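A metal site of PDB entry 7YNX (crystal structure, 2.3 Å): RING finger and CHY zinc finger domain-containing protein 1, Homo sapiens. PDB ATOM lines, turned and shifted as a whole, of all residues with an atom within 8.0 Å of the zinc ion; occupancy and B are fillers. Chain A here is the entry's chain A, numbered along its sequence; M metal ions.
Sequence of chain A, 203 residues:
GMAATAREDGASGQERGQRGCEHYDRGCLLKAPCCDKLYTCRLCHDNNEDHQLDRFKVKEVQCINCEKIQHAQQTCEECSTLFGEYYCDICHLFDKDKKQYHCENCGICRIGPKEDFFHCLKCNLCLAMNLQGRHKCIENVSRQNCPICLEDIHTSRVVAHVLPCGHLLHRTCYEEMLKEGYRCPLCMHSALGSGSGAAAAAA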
ATOM      1  N   ILE A 138      16.830  14.563  -9.233  1.00  0.00           N
ATOM      2  CA  ILE A 138      17.311  14.427 -10.601  1.00  0.00           C
ATOM      3  C   ILE A 138      16.568  15.434 -11.460  1.00  0.00           C
ATOM      4  O   ILE A 138      15.334  15.496 -11.414  1.00  0.00           O
ATOM      5  CB  ILE A 138      17.126  12.996 -11.153  1.00  0.00           C
ATOM      6  CG1 ILE A 138      17.799  11.989 -10.238  1.00  0.00           C
ATOM      7  CG2 ILE A 138      17.658  12.909 -12.599  1.00  0.00           C
ATOM      8  CD1 ILE A 138      17.520  10.540 -10.580  1.00  0.00           C
ATOM      9  N   PRO A 147      10.739   4.328 -16.826  1.00  0.00           N
ATOM     10  CA  PRO A 147      11.635   3.417 -17.548  1.00  0.00           C
ATOM     11  C   PRO A 147      11.045   2.026 -17.758  1.00  0.00           C
ATOM     12  O   PRO A 147      11.521   1.292 -18.627  1.00  0.00           O
ATOM     13  CB  PRO A 147      12.910   3.366 -16.690  1.00  0.00           C
ATOM     14  CG  PRO A 147      12.493   3.842 -15.371  1.00  0.00           C
ATOM     15  CD  PRO A 147      11.377   4.834 -15.586  1.00  0.00           C
ATOM     16  N   LEU A 163      12.383   6.335  -6.061  1.00  0.00           N
ATOM     17  CA  LEU A 163      13.317   5.357  -5.568  1.00  0.00           C
ATOM     18  C   LEU A 163      14.401   6.053  -4.758  1.00  0.00           C
ATOM     19  O   LEU A 163      14.615   7.264  -4.904  1.00  0.00           O
ATOM     20  CB  LEU A 163      13.918   4.563  -6.732  1.00  0.00           C
ATOM     21  CG  LEU A 163      12.961   3.593  -7.429  1.00  0.00           C
ATOM     22  CD1 LEU A 163      13.502   3.206  -8.790  1.00  0.00           C
ATOM     23  CD2 LEU A 163      12.682   2.348  -6.579  1.00  0.00           C
ATOM     24  N   PRO A 164      15.062   5.331  -3.873  1.00  0.00           N
ATOM     25  CA  PRO A 164      16.137   5.947  -3.074  1.00  0.00           C
ATOM     26  C   PRO A 164      17.219   6.611  -3.930  1.00  0.00           C
ATOM     27  O   PRO A 164      17.894   7.533  -3.466  1.00  0.00           O
ATOM     28  CB  PRO A 164      16.708   4.774  -2.260  1.00  0.00           C
ATOM     29  CG  PRO A 164      16.115   3.517  -2.875  1.00  0.00           C
ATOM     30  CD  PRO A 164      14.794   3.949  -3.450  1.00  0.00           C
ATOM     31  N   CYS A 165      17.388   6.170  -5.171  1.00  0.00           N
ATOM     32  CA  CYS A 165      18.339   6.794  -6.091  1.00  0.00           C
ATOM     33  C   CYS A 165      17.802   8.070  -6.749  1.00  0.00           C
ATOM     34  O   CYS A 165      18.565   8.770  -7.426  1.00  0.00           O
ATOM     35  CB  CYS A 165      18.725   5.795  -7.182  1.00  0.00           C
ATOM     36  SG  CYS A 165      17.297   5.209  -8.129  1.00  0.00           S
ATOM     37  N   GLY A 166      16.513   8.374  -6.583  1.00  0.00           N
ATOM     38  CA  GLY A 166      15.900   9.557  -7.153  1.00  0.00           C
ATOM     39  C   GLY A 166      15.187   9.306  -8.462  1.00  0.00           C
ATOM     40  O   GLY A 166      14.589  10.236  -9.015  1.00  0.00           O
ATOM     41  N   HIS A 167      15.262   8.091  -8.994  1.00  0.00           N
ATOM     42  CA  HIS A 167      14.530   7.788 -10.211  1.00  0.00           C
ATOM     43  C   HIS A 167      13.083   7.475  -9.857  1.00  0.00           C
ATOM     44  O   HIS A 167      12.773   6.997  -8.752  1.00  0.00           O
ATOM     45  CB  HIS A 167      15.178   6.618 -10.936  1.00  0.00           C
ATOM     46  CG  HIS A 167      16.386   7.001 -11.736  1.00  0.00           C
ATOM     47  ND1 HIS A 167      17.674   6.749 -11.308  1.00  0.00           N
ATOM     48  CD2 HIS A 167      16.499   7.585 -12.950  1.00  0.00           C
ATOM     49  CE1 HIS A 167      18.526   7.171 -12.221  1.00  0.00           C
ATOM     50  NE2 HIS A 167      17.846   7.687 -13.232  1.00  0.00           N
ATOM     51  N   LEU A 168      12.175   7.734 -10.802  1.00  0.00           N
ATOM     52  CA  LEU A 168      10.733   7.663 -10.561  1.00  0.00           C
ATOM     53  C   LEU A 168      10.103   6.542 -11.380  1.00  0.00           C
ATOM     54  O   LEU A 168      10.402   6.412 -12.575  1.00  0.00           O
ATOM     55  CB  LEU A 168      10.059   8.992 -10.899  1.00  0.00           C
ATOM     56  CG  LEU A 168      10.237  10.164  -9.940  1.00  0.00           C
ATOM     57  CD1 LEU A 168       9.806  11.475 -10.595  1.00  0.00           C
ATOM     58  CD2 LEU A 168       9.452   9.918  -8.666  1.00  0.00           C
ATOM     59  N   LEU A 169       9.231   5.774 -10.740  1.00  0.00           N
ATOM     60  CA  LEU A 169       8.461   4.712 -11.387  1.00  0.00           C
ATOM     61  C   LEU A 169       6.997   4.880 -11.009  1.00  0.00           C
ATOM     62  O   LEU A 169       6.686   5.363  -9.921  1.00  0.00           O
ATOM     63  CB  LEU A 169       8.934   3.306 -10.940  1.00  0.00           C
ATOM     64  CG  LEU A 169      10.408   2.938 -11.107  1.00  0.00           C
ATOM     65  CD1 LEU A 169      10.676   1.586 -10.545  1.00  0.00           C
ATOM     66  CD2 LEU A 169      10.754   2.956 -12.576  1.00  0.00           C
ATOM     67  N   ARG A 183      16.001  -3.725  -7.996  1.00  0.00           N
ATOM     68  CA  ARG A 183      16.978  -2.703  -8.318  1.00  0.00           C
ATOM     69  C   ARG A 183      16.350  -1.704  -9.270  1.00  0.00           C
ATOM     70  O   ARG A 183      15.434  -2.040 -10.027  1.00  0.00           O
ATOM     71  CB  ARG A 183      18.243  -3.289  -8.963  1.00  0.00           C
ATOM     72  CG  ARG A 183      19.119  -4.057  -8.003  1.00  0.00           C
ATOM     73  CD  ARG A 183      20.307  -4.761  -8.702  1.00  0.00           C
ATOM     74  NE  ARG A 183      21.144  -5.433  -7.706  1.00  0.00           N
ATOM     75  CZ  ARG A 183      21.984  -4.793  -6.894  1.00  0.00           C
ATOM     76  NH1 ARG A 183      22.123  -3.468  -6.972  1.00  0.00           N
ATOM     77  NH2 ARG A 183      22.686  -5.472  -5.991  1.00  0.00           N
ATOM     78  N   CYS A 184      16.876  -0.483  -9.247  1.00  0.00           N
ATOM     79  CA  CYS A 184      16.369   0.539 -10.144  1.00  0.00           C
ATOM     80  C   CYS A 184      16.599   0.109 -11.592  1.00  0.00           C
ATOM     81  O   CYS A 184      17.726  -0.303 -11.945  1.00  0.00           O
ATOM     82  CB  CYS A 184      17.039   1.877  -9.906  1.00  0.00           C
ATOM     83  SG  CYS A 184      16.543   3.050 -11.208  1.00  0.00           S
ATOM     84  N   PRO A 185      15.579   0.167 -12.446  1.00  0.00           N
ATOM     85  CA  PRO A 185      15.735  -0.300 -13.838  1.00  0.00           C
ATOM     86  C   PRO A 185      16.720   0.512 -14.639  1.00  0.00           C
ATOM     87  O   PRO A 185      17.219   0.027 -15.656  1.00  0.00           O
ATOM     88  CB  PRO A 185      14.315  -0.150 -14.402  1.00  0.00           C
ATOM     89  CG  PRO A 185      13.429  -0.235 -13.233  1.00  0.00           C
ATOM     90  CD  PRO A 185      14.171   0.398 -12.083  1.00  0.00           C
ATOM     91  N   LEU A 186      17.012   1.743 -14.227  1.00  0.00           N
ATOM     92  CA  LEU A 186      17.962   2.574 -14.951  1.00  0.00           C
ATOM     93  C   LEU A 186      19.350   2.449 -14.350  1.00  0.00           C
ATOM     94  O   LEU A 186      20.294   2.013 -15.017  1.00  0.00           O
ATOM     95  CB  LEU A 186      17.493   4.029 -14.949  1.00  0.00           C
ATOM     96  CG  LEU A 186      16.422   4.326 -15.991  1.00  0.00           C
ATOM     97  CD1 LEU A 186      15.876   5.755 -15.852  1.00  0.00           C
ATOM     98  CD2 LEU A 186      16.963   4.060 -17.382  1.00  0.00           C
ATOM     99  N   CYS A 187      19.514   2.822 -13.082  1.00  0.00           N
ATOM    100  CA  CYS A 187      20.843   2.952 -12.521  1.00  0.00           C
ATOM    101  C   CYS A 187      21.265   1.727 -11.703  1.00  0.00           C
ATOM    102  O   CYS A 187      22.378   1.704 -11.182  1.00  0.00           O
ATOM    103  CB  CYS A 187      20.931   4.225 -11.688  1.00  0.00           C
ATOM    104  SG  CYS A 187      20.189   4.071 -10.061  1.00  0.00           S
ATOM    105  N   MET A 188      20.394   0.719 -11.598  1.00  0.00           N
ATOM    106  CA  MET A 188      20.676  -0.576 -11.016  1.00  0.00           C
ATOM    107  C   MET A 188      20.933  -0.522  -9.513  1.00  0.00           C
ATOM    108  O   MET A 188      21.115  -1.580  -8.891  1.00  0.00           O
ATOM    109  CB  MET A 188      21.854  -1.289 -11.710  1.00  0.00           C
ATOM    110  CG  MET A 188      21.507  -1.780 -13.120  1.00  0.00           C
ATOM    111  SD  MET A 188      20.056  -2.861 -13.119  1.00  0.00           S
ATOM    112  CE  MET A 188      20.827  -4.403 -12.623  1.00  0.00           C
ATOM    113  N   HIS A 189      20.947   0.657  -8.899  1.00  0.00           N
ATOM    114  CA  HIS A 189      20.981   0.730  -7.436  1.00  0.00           C
ATOM    115  C   HIS A 189      19.790   0.007  -6.843  1.00  0.00           C
ATOM    116  O   HIS A 189      18.700  -0.036  -7.436  1.00  0.00           O
ATOM    117  CB  HIS A 189      20.991   2.174  -6.968  1.00  0.00           C
ATOM    118  CG  HIS A 189      22.353   2.754  -6.833  1.00  0.00           C
ATOM    119  ND1 HIS A 189      23.014   3.345  -7.883  1.00  0.00           N
ATOM    120  CD2 HIS A 189      23.201   2.810  -5.775  1.00  0.00           C
ATOM    121  CE1 HIS A 189      24.205   3.753  -7.475  1.00  0.00           C
ATOM    122  NE2 HIS A 189      24.340   3.435  -6.200  1.00  0.00           N
ATOM    123  N   SER A 190      19.993  -0.581  -5.677  1.00  0.00           N
ATOM    124  CA  SER A 190      18.914  -1.279  -4.999  1.00  0.00           C
ATOM    125  C   SER A 190      17.856  -0.293  -4.535  1.00  0.00           C
ATOM    126  O   SER A 190      18.145   0.854  -4.202  1.00  0.00           O
ATOM    127  CB  SER A 190      19.447  -2.052  -3.802  1.00  0.00           C
ATOM    128  OG  SER A 190      18.365  -2.573  -3.039  1.00  0.00           O
HETATM  129 ZN    ZN M   1      17.906   4.716 -10.442  1.00  0.00          ZN
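The backbone NH of Leu 186 sits close to the side-chain sulfur of Cys 184 (3.3 Å). SG of Cys 187 sits close to ND1 of His 189, at 3.6 Å. The backbone NH of Cys 184 is in hydrogen-bond range of the backbone carbonyl oxygen of His 189 (2.6 Å).
The zinc ion is bound by ND1 of His 167, SG of Cys 184, SG of Cys 187 and SG of Cys 165.
Within 4 Å of the zinc ion: Cys 165, His 167, Cys 184 and Cys 187. The nearest printed residue that does not touch the zinc ion is Leu 186 (4.6 Å).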
